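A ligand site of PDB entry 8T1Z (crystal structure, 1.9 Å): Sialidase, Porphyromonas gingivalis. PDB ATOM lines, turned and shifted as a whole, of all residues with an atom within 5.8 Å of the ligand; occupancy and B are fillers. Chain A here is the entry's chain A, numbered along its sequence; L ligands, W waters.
OD2 of Asp 364 sits at hydrogen-bond distance from O8 of the ligand, at 2.5 Å.
An oxygen (O3) of the ligand sits at hydrogen-bond distance from the side-chain carboxylate of Asp 202 (2.5 Å).
OD1 of Asp 239 is in hydrogen-bond range of O4 of the ligand (2.7 Å).
An oxygen (O1) of the ligand lies within salt-bridge range of the guanidinium group (NH1) of Arg 177, at 2.8 Å.
An oxygen (O1) of the ligand lies within salt-bridge range of the guanidinium group of Arg 443.
O5 of the ligand sits at hydrogen-bond distance from OH of Tyr 471 (2.9 Å).
An oxygen (O2) of the ligand lies within salt-bridge range of the guanidinium group of Arg 381.
NH2 of Arg 196 sits at hydrogen-bond distance from O4 of the ligand, 3.1 Å away.
The side-chain carboxylate (OE2) of Glu 365 is in hydrogen-bond range of an oxygen (O7) of the ligand, at 3.5 Å.
The side-chain carboxylate (OD1) of Asp 364 is in salt-bridge range of the guanidinium group (NE) of Arg 381, at 3.9 Å.
The side-chain carboxylate (OD1) of Asp 202 is in salt-bridge range of the guanidinium group (NH1) of Arg 196, at 2.7 Å.
N of Asp 194 lies within hydrogen-bond range of O of Arg 177, 2.6 Å away.
The guanidinium group (NE) of Arg 177 is in salt-bridge range of the side-chain carboxylate (OE2) of Glu 487, at 2.8 Å.
N of Tyr 471 is in hydrogen-bond range of OE1 of Glu 487.
The guanidinium group (NH2) of Arg 381 lies within hydrogen-bond range of the side-chain amide oxygen (OE1) of Gln 383 (2.8 Å).
The guanidinium group (NE) of Arg 381 lies within hydrogen-bond range of the backbone carbonyl oxygen (O) of Gly 416, 3.2 Å away.
The guanidinium group (NH2) of Arg 196 is in salt-bridge range of the side-chain carboxylate (OD2) of Asp 194 (2.9 Å).
Merely in contact with the ligand: Ile 178 (3.8 Å), Leu 260 (3.6 Å), Phe 310 (3.6 Å) and Gln 383 (3.8 Å).
Hydrophobic or aromatic side chains that line the ligand: Ile 178, Leu 260, Phe 310 and Tyr 471.
Of the 21 residues printed, 13 come within 4 Å of the ligand.
The nearest printed residue that does not touch the ligand is Val 255 (4.1 Å).
Water W4 lies within hydrogen-bond range of O9 of the ligand, N of Leu 260 and O of Leu 203.
Water W2 bridges an oxygen (O6) of the ligand and the indole nitrogen (NE1) of Trp 261.
Water W3 lies within hydrogen-bond range of an oxygen (O4) of the ligand (2.9 Å), the backbone NH of Leu 203 (3.2 Å) and the guanidinium group of Arg 196 (3.4 Å).
Water W1 lies within hydrogen-bond range of the side-chain carboxylate (OD2) of Asp 202 (3.2 Å) and an oxygen (O6) of the ligand (3.2 Å).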
ATOM      1  N   ARG A 177     -10.242 -16.299  -7.420  1.00  0.00           N
ATOM      2  CA  ARG A 177     -10.629 -17.075  -6.257  1.00  0.00           C
ATOM      3  C   ARG A 177      -9.362 -17.396  -5.484  1.00  0.00           C
ATOM      4  O   ARG A 177      -8.249 -17.306  -6.017  1.00  0.00           O
ATOM      5  CB  ARG A 177     -11.372 -18.376  -6.647  1.00  0.00           C
ATOM      6  CG  ARG A 177     -12.891 -18.248  -6.726  1.00  0.00           C
ATOM      7  CD  ARG A 177     -13.603 -19.500  -6.296  1.00  0.00           C
ATOM      8  NE  ARG A 177     -13.520 -19.639  -4.849  1.00  0.00           N
ATOM      9  CZ  ARG A 177     -13.783 -20.768  -4.193  1.00  0.00           C
ATOM     10  NH1 ARG A 177     -14.204 -21.846  -4.843  1.00  0.00           N
ATOM     11  NH2 ARG A 177     -13.613 -20.816  -2.868  1.00  0.00           N
ATOM     12  N   ILE A 178      -9.548 -17.822  -4.235  1.00  0.00           N
ATOM     13  CA  ILE A 178      -8.527 -18.482  -3.395  1.00  0.00           C
ATOM     14  C   ILE A 178      -7.460 -17.499  -2.895  1.00  0.00           C
ATOM     15  O   ILE A 178      -6.305 -17.556  -3.322  1.00  0.00           O
ATOM     16  CB  ILE A 178      -7.875 -19.667  -4.118  1.00  0.00           C
ATOM     17  CG1 ILE A 178      -8.911 -20.531  -4.821  1.00  0.00           C
ATOM     18  CG2 ILE A 178      -7.172 -20.561  -3.123  1.00  0.00           C
ATOM     19  CD1 ILE A 178      -9.978 -21.087  -3.898  1.00  0.00           C
ATOM     20  N   ASP A 194      -5.873 -17.380  -7.178  1.00  0.00           N
ATOM     21  CA  ASP A 194      -6.116 -18.069  -8.435  1.00  0.00           C
ATOM     22  C   ASP A 194      -6.614 -17.049  -9.442  1.00  0.00           C
ATOM     23  O   ASP A 194      -7.630 -16.381  -9.205  1.00  0.00           O
ATOM     24  CB  ASP A 194      -7.193 -19.157  -8.343  1.00  0.00           C
ATOM     25  CG  ASP A 194      -6.748 -20.372  -7.588  1.00  0.00           C
ATOM     26  OD1 ASP A 194      -5.578 -20.469  -7.148  1.00  0.00           O
ATOM     27  OD2 ASP A 194      -7.557 -21.326  -7.606  1.00  0.00           O
ATOM     28  N   ARG A 196      -8.593 -17.256 -12.258  1.00  0.00           N
ATOM     29  CA  ARG A 196      -9.504 -18.231 -12.870  1.00  0.00           C
ATOM     30  C   ARG A 196      -9.977 -17.664 -14.213  1.00  0.00           C
ATOM     31  O   ARG A 196     -11.057 -17.077 -14.314  1.00  0.00           O
ATOM     32  CB  ARG A 196     -10.637 -18.559 -11.907  1.00  0.00           C
ATOM     33  CG  ARG A 196     -10.139 -19.147 -10.570  1.00  0.00           C
ATOM     34  CD  ARG A 196     -10.997 -20.238  -9.966  1.00  0.00           C
ATOM     35  NE  ARG A 196     -10.282 -21.057  -8.969  1.00  0.00           N
ATOM     36  CZ  ARG A 196     -10.831 -22.000  -8.205  1.00  0.00           C
ATOM     37  NH1 ARG A 196     -12.136 -22.208  -8.184  1.00  0.00           N
ATOM     38  NH2 ARG A 196     -10.037 -22.746  -7.431  1.00  0.00           N
ATOM     39  N   ASP A 202     -12.823 -25.021 -10.159  1.00  0.00           N
ATOM     40  CA  ASP A 202     -11.530 -25.481  -9.639  1.00  0.00           C
ATOM     41  C   ASP A 202     -10.738 -26.210 -10.730  1.00  0.00           C
ATOM     42  O   ASP A 202     -11.246 -26.472 -11.824  1.00  0.00           O
ATOM     43  CB  ASP A 202     -11.706 -26.461  -8.469  1.00  0.00           C
ATOM     44  CG  ASP A 202     -12.574 -25.917  -7.339  1.00  0.00           C
ATOM     45  OD1 ASP A 202     -12.681 -24.687  -7.140  1.00  0.00           O
ATOM     46  OD2 ASP A 202     -13.106 -26.767  -6.581  1.00  0.00           O
ATOM     47  N   LEU A 203      -9.492 -26.535 -10.429  1.00  0.00           N
ATOM     48  CA  LEU A 203      -8.762 -27.528 -11.204  1.00  0.00           C
ATOM     49  C   LEU A 203      -9.659 -28.765 -11.392  1.00  0.00           C
ATOM     50  O   LEU A 203     -10.327 -29.177 -10.439  1.00  0.00           O
ATOM     51  CB  LEU A 203      -7.476 -27.923 -10.459  1.00  0.00           C
ATOM     52  CG  LEU A 203      -6.391 -26.857 -10.306  1.00  0.00           C
ATOM     53  CD1 LEU A 203      -5.332 -27.261  -9.290  1.00  0.00           C
ATOM     54  CD2 LEU A 203      -5.745 -26.526 -11.647  1.00  0.00           C
ATOM     55  N   ASP A 239      -4.381 -22.847  -5.679  1.00  0.00           N
ATOM     56  CA  ASP A 239      -4.427 -23.167  -4.242  1.00  0.00           C
ATOM     57  C   ASP A 239      -3.070 -22.903  -3.567  1.00  0.00           C
ATOM     58  O   ASP A 239      -2.411 -23.802  -3.061  1.00  0.00           O
ATOM     59  CB  ASP A 239      -4.869 -24.622  -3.997  1.00  0.00           C
ATOM     60  CG  ASP A 239      -6.383 -24.767  -3.896  1.00  0.00           C
ATOM     61  OD1 ASP A 239      -7.098 -24.205  -4.729  1.00  0.00           O
ATOM     62  OD2 ASP A 239      -6.847 -25.473  -2.965  1.00  0.00           O
ATOM     63  N   VAL A 255      -0.731 -26.535  -5.920  1.00  0.00           N
ATOM     64  CA  VAL A 255      -0.942 -27.738  -6.722  1.00  0.00           C
ATOM     65  C   VAL A 255      -1.146 -27.343  -8.177  1.00  0.00           C
ATOM     66  O   VAL A 255      -1.379 -26.182  -8.518  1.00  0.00           O
ATOM     67  CB  VAL A 255      -2.121 -28.602  -6.227  1.00  0.00           C
ATOM     68  CG1 VAL A 255      -1.784 -29.347  -4.894  1.00  0.00           C
ATOM     69  CG2 VAL A 255      -3.368 -27.759  -6.080  1.00  0.00           C
ATOM     70  N   LEU A 260      -8.600 -32.715  -7.869  1.00  0.00           N
ATOM     71  CA  LEU A 260      -8.341 -33.434  -6.633  1.00  0.00           C
ATOM     72  C   LEU A 260      -8.828 -34.876  -6.679  1.00  0.00           C
ATOM     73  O   LEU A 260      -8.070 -35.816  -6.386  1.00  0.00           O
ATOM     74  CB  LEU A 260      -9.001 -32.683  -5.482  1.00  0.00           C
ATOM     75  CG  LEU A 260      -9.019 -33.325  -4.096  1.00  0.00           C
ATOM     76  CD1 LEU A 260      -7.605 -33.489  -3.567  1.00  0.00           C
ATOM     77  CD2 LEU A 260      -9.840 -32.437  -3.182  1.00  0.00           C
ATOM     78  N   TRP A 261     -10.088 -35.086  -7.030  1.00  0.00           N
ATOM     79  CA  TRP A 261     -10.687 -36.416  -7.072  1.00  0.00           C
ATOM     80  C   TRP A 261     -10.333 -37.202  -8.330  1.00  0.00           C
ATOM     81  O   TRP A 261     -10.729 -38.375  -8.449  1.00  0.00           O
ATOM     82  CB  TRP A 261     -12.212 -36.290  -6.923  1.00  0.00           C
ATOM     83  CG  TRP A 261     -12.549 -35.442  -5.692  1.00  0.00           C
ATOM     84  CD1 TRP A 261     -13.053 -34.166  -5.684  1.00  0.00           C
ATOM     85  CD2 TRP A 261     -12.337 -35.806  -4.316  1.00  0.00           C
ATOM     86  NE1 TRP A 261     -13.173 -33.718  -4.371  1.00  0.00           N
ATOM     87  CE2 TRP A 261     -12.753 -34.707  -3.527  1.00  0.00           C
ATOM     88  CE3 TRP A 261     -11.851 -36.945  -3.672  1.00  0.00           C
ATOM     89  CZ2 TRP A 261     -12.711 -34.731  -2.129  1.00  0.00           C
ATOM     90  CZ3 TRP A 261     -11.806 -36.960  -2.278  1.00  0.00           C
ATOM     91  CH2 TRP A 261     -12.234 -35.864  -1.530  1.00  0.00           C
ATOM     92  N   GLN A 269      -2.263 -35.200  -9.234  1.00  0.00           N
ATOM     93  CA  GLN A 269      -2.255 -33.757  -9.091  1.00  0.00           C
ATOM     94  C   GLN A 269      -1.039 -33.417  -8.254  1.00  0.00           C
ATOM     95  O   GLN A 269      -0.887 -33.961  -7.156  1.00  0.00           O
ATOM     96  CB  GLN A 269      -3.538 -33.277  -8.420  1.00  0.00           C
ATOM     97  CG  GLN A 269      -3.552 -31.779  -8.111  1.00  0.00           C
ATOM     98  CD  GLN A 269      -4.755 -31.392  -7.285  1.00  0.00           C
ATOM     99  OE1 GLN A 269      -4.854 -31.732  -6.092  1.00  0.00           O
ATOM    100  NE2 GLN A 269      -5.739 -30.763  -7.935  1.00  0.00           N
ATOM    101  N   PHE A 310      -3.201 -32.067  -1.076  1.00  0.00           N
ATOM    102  CA  PHE A 310      -3.088 -30.631  -1.301  1.00  0.00           C
ATOM    103  C   PHE A 310      -3.041 -29.907   0.034  1.00  0.00           C
ATOM    104  O   PHE A 310      -3.718 -30.279   0.994  1.00  0.00           O
ATOM    105  CB  PHE A 310      -4.203 -30.111  -2.214  1.00  0.00           C
ATOM    106  CG  PHE A 310      -5.529 -29.843  -1.542  1.00  0.00           C
ATOM    107  CD1 PHE A 310      -6.380 -30.891  -1.204  1.00  0.00           C
ATOM    108  CD2 PHE A 310      -5.977 -28.528  -1.352  1.00  0.00           C
ATOM    109  CE1 PHE A 310      -7.633 -30.652  -0.628  1.00  0.00           C
ATOM    110  CE2 PHE A 310      -7.224 -28.273  -0.761  1.00  0.00           C
ATOM    111  CZ  PHE A 310      -8.064 -29.356  -0.390  1.00  0.00           C
ATOM    112  N   LEU A 339     -10.773 -37.389   2.913  1.00  0.00           N
ATOM    113  CA  LEU A 339      -9.404 -36.912   3.093  1.00  0.00           C
ATOM    114  C   LEU A 339      -8.960 -37.062   4.549  1.00  0.00           C
ATOM    115  O   LEU A 339      -9.771 -36.940   5.467  1.00  0.00           O
ATOM    116  CB  LEU A 339      -9.273 -35.440   2.701  1.00  0.00           C
ATOM    117  CG  LEU A 339      -9.689 -35.089   1.260  1.00  0.00           C
ATOM    118  CD1 LEU A 339      -9.580 -33.602   1.048  1.00  0.00           C
ATOM    119  CD2 LEU A 339      -8.834 -35.825   0.250  1.00  0.00           C
ATOM    120  N   ASP A 364     -10.335 -31.905   6.094  1.00  0.00           N
ATOM    121  CA  ASP A 364     -10.255 -31.170   4.837  1.00  0.00           C
ATOM    122  C   ASP A 364      -9.236 -30.049   5.021  1.00  0.00           C
ATOM    123  O   ASP A 364      -8.340 -30.185   5.870  1.00  0.00           O
ATOM    124  CB  ASP A 364     -11.637 -30.633   4.440  1.00  0.00           C
ATOM    125  CG  ASP A 364     -11.772 -30.456   2.942  1.00  0.00           C
ATOM    126  OD1 ASP A 364     -11.222 -29.457   2.415  1.00  0.00           O
ATOM    127  OD2 ASP A 364     -12.408 -31.314   2.290  1.00  0.00           O
ATOM    128  N   GLU A 365      -9.329 -28.950   4.263  1.00  0.00           N
ATOM    129  CA  GLU A 365      -8.378 -27.844   4.419  1.00  0.00           C
ATOM    130  C   GLU A 365      -8.185 -27.511   5.885  1.00  0.00           C
ATOM    131  O   GLU A 365      -9.152 -27.233   6.590  1.00  0.00           O
ATOM    132  CB  GLU A 365      -8.875 -26.596   3.680  1.00  0.00           C
ATOM    133  CG  GLU A 365      -8.991 -26.774   2.154  1.00  0.00           C
ATOM    134  CD  GLU A 365      -9.881 -25.731   1.537  1.00  0.00           C
ATOM    135  OE1 GLU A 365     -10.781 -25.230   2.256  1.00  0.00           O
ATOM    136  OE2 GLU A 365      -9.715 -25.442   0.322  1.00  0.00           O
ATOM    137  N   ARG A 381     -11.291 -27.771   8.431  1.00  0.00           N
ATOM    138  CA  ARG A 381     -12.590 -27.532   7.814  1.00  0.00           C
ATOM    139  C   ARG A 381     -13.474 -28.784   7.943  1.00  0.00           C
ATOM    140  O   ARG A 381     -13.011 -29.906   7.740  1.00  0.00           O
ATOM    141  CB  ARG A 381     -12.417 -27.168   6.331  1.00  0.00           C
ATOM    142  CG  ARG A 381     -13.572 -27.543   5.401  1.00  0.00           C
ATOM    143  CD  ARG A 381     -13.495 -26.676   4.137  1.00  0.00           C
ATOM    144  NE  ARG A 381     -14.280 -27.161   3.016  1.00  0.00           N
ATOM    145  CZ  ARG A 381     -14.128 -26.743   1.753  1.00  0.00           C
ATOM    146  NH1 ARG A 381     -13.247 -25.804   1.442  1.00  0.00           N
ATOM    147  NH2 ARG A 381     -14.865 -27.288   0.789  1.00  0.00           N
ATOM    148  N   GLN A 383     -15.981 -30.861   6.268  1.00  0.00           N
ATOM    149  CA  GLN A 383     -16.461 -31.150   4.921  1.00  0.00           C
ATOM    150  C   GLN A 383     -17.479 -32.282   4.947  1.00  0.00           C
ATOM    151  O   GLN A 383     -17.222 -33.343   5.538  1.00  0.00           O
ATOM    152  CB  GLN A 383     -15.301 -31.501   3.991  1.00  0.00           C
ATOM    153  CG  GLN A 383     -15.703 -31.731   2.545  1.00  0.00           C
ATOM    154  CD  GLN A 383     -16.346 -30.525   1.897  1.00  0.00           C
ATOM    155  OE1 GLN A 383     -16.099 -29.379   2.274  1.00  0.00           O
ATOM    156  NE2 GLN A 383     -17.164 -30.779   0.875  1.00  0.00           N
ATOM    157  N   GLY A 416     -18.478 -25.342   5.891  1.00  0.00           N
ATOM    158  CA  GLY A 416     -17.651 -26.146   5.019  1.00  0.00           C
ATOM    159  C   GLY A 416     -16.778 -25.234   4.191  1.00  0.00           C
ATOM    160  O   GLY A 416     -16.883 -25.219   2.967  1.00  0.00           O
ATOM    161  N   ARG A 443     -22.250 -20.099   2.359  1.00  0.00           N
ATOM    162  CA  ARG A 443     -21.103 -19.197   2.329  1.00  0.00           C
ATOM    163  C   ARG A 443     -21.636 -17.768   2.281  1.00  0.00           C
ATOM    164  O   ARG A 443     -21.774 -17.146   1.217  1.00  0.00           O
ATOM    165  CB  ARG A 443     -20.184 -19.533   1.166  1.00  0.00           C
ATOM    166  CG  ARG A 443     -19.293 -20.726   1.484  1.00  0.00           C
ATOM    167  CD  ARG A 443     -18.676 -21.370   0.265  1.00  0.00           C
ATOM    168  NE  ARG A 443     -17.890 -22.537   0.652  1.00  0.00           N
ATOM    169  CZ  ARG A 443     -16.858 -23.019  -0.038  1.00  0.00           C
ATOM    170  NH1 ARG A 443     -16.459 -22.446  -1.168  1.00  0.00           N
ATOM    171  NH2 ARG A 443     -16.207 -24.081   0.424  1.00  0.00           N
ATOM    172  N   TYR A 471     -13.800 -17.997   1.212  1.00  0.00           N
ATOM    173  CA  TYR A 471     -12.468 -18.190   1.775  1.00  0.00           C
ATOM    174  C   TYR A 471     -11.947 -16.872   2.318  1.00  0.00           C
ATOM    175  O   TYR A 471     -12.199 -15.795   1.742  1.00  0.00           O
ATOM    176  CB  TYR A 471     -11.500 -18.718   0.723  1.00  0.00           C
ATOM    177  CG  TYR A 471     -11.587 -20.205   0.423  1.00  0.00           C
ATOM    178  CD1 TYR A 471     -12.756 -20.915   0.652  1.00  0.00           C
ATOM    179  CD2 TYR A 471     -10.478 -20.895  -0.067  1.00  0.00           C
ATOM    180  CE1 TYR A 471     -12.826 -22.278   0.389  1.00  0.00           C
ATOM    181  CE2 TYR A 471     -10.540 -22.265  -0.339  1.00  0.00           C
ATOM    182  CZ  TYR A 471     -11.720 -22.944  -0.099  1.00  0.00           C
ATOM    183  OH  TYR A 471     -11.777 -24.298  -0.357  1.00  0.00           O
ATOM    184  N   GLU A 487     -12.962 -13.555   0.007  1.00  0.00           N
ATOM    185  CA  GLU A 487     -13.783 -13.738  -1.193  1.00  0.00           C
ATOM    186  C   GLU A 487     -15.161 -13.125  -0.961  1.00  0.00           C
ATOM    187  O   GLU A 487     -15.948 -13.647  -0.165  1.00  0.00           O
ATOM    188  CB  GLU A 487     -13.922 -15.223  -1.497  1.00  0.00           C
ATOM    189  CG  GLU A 487     -12.590 -15.954  -1.721  1.00  0.00           C
ATOM    190  CD  GLU A 487     -12.770 -17.349  -2.292  1.00  0.00           C
ATOM    191  OE1 GLU A 487     -13.427 -18.190  -1.650  1.00  0.00           O
ATOM    192  OE2 GLU A 487     -12.251 -17.596  -3.413  1.00  0.00           O
HETATM  193  C1  LIG L   1     -14.111 -24.800  -2.416  1.00  0.00           C
HETATM  194  C2  LIG L   1     -12.921 -25.518  -3.155  1.00  0.00           C
HETATM  195  C3  LIG L   1     -11.905 -24.558  -3.773  1.00  0.00           C
HETATM  196  C4  LIG L   1     -10.465 -25.082  -3.832  1.00  0.00           C
HETATM  197  C5  LIG L   1     -10.425 -26.621  -3.772  1.00  0.00           C
HETATM  198  C6  LIG L   1     -11.087 -27.109  -2.466  1.00  0.00           C
HETATM  199  C7  LIG L   1     -11.420 -28.634  -2.469  1.00  0.00           C
HETATM  200  C8  LIG L   1     -12.107 -29.064  -1.150  1.00  0.00           C
HETATM  201  C9  LIG L   1     -12.050 -30.589  -1.043  1.00  0.00           C
HETATM  202  C10 LIG L   1      -8.690 -28.152  -4.725  1.00  0.00           C
HETATM  203  C11 LIG L   1      -7.202 -28.473  -4.858  1.00  0.00           C
HETATM  204  N1  LIG L   1      -9.032 -27.083  -3.957  1.00  0.00           N
HETATM  205  O1  LIG L   1     -14.368 -23.615  -2.742  1.00  0.00           O
HETATM  206  O2  LIG L   1     -14.650 -25.573  -1.590  1.00  0.00           O
HETATM  207  O3  LIG L   1     -13.475 -26.358  -4.105  1.00  0.00           O
HETATM  208  O4  LIG L   1      -9.790 -24.662  -5.027  1.00  0.00           O
HETATM  209  O5  LIG L   1     -12.324 -26.447  -2.207  1.00  0.00           O
HETATM  210  O6  LIG L   1     -12.202 -29.041  -3.588  1.00  0.00           O
HETATM  211  O7  LIG L   1     -11.478 -28.404  -0.042  1.00  0.00           O
HETATM  212  O8  LIG L   1     -13.061 -31.024  -0.143  1.00  0.00           O
HETATM  213  O9  LIG L   1      -9.505 -28.880  -5.273  1.00  0.00           O
HETATM  214  O   HOH W   1     -12.361 -29.879  -6.690  1.00  0.00           O
HETATM  215  O   HOH W   2     -14.070 -30.867  -4.291  1.00  0.00           O
HETATM  216  O   HOH W   3      -8.674 -25.892  -7.439  1.00  0.00           O
HETATM  217  O   HOH W   4      -9.166 -29.920  -7.641  1.00  0.00           O
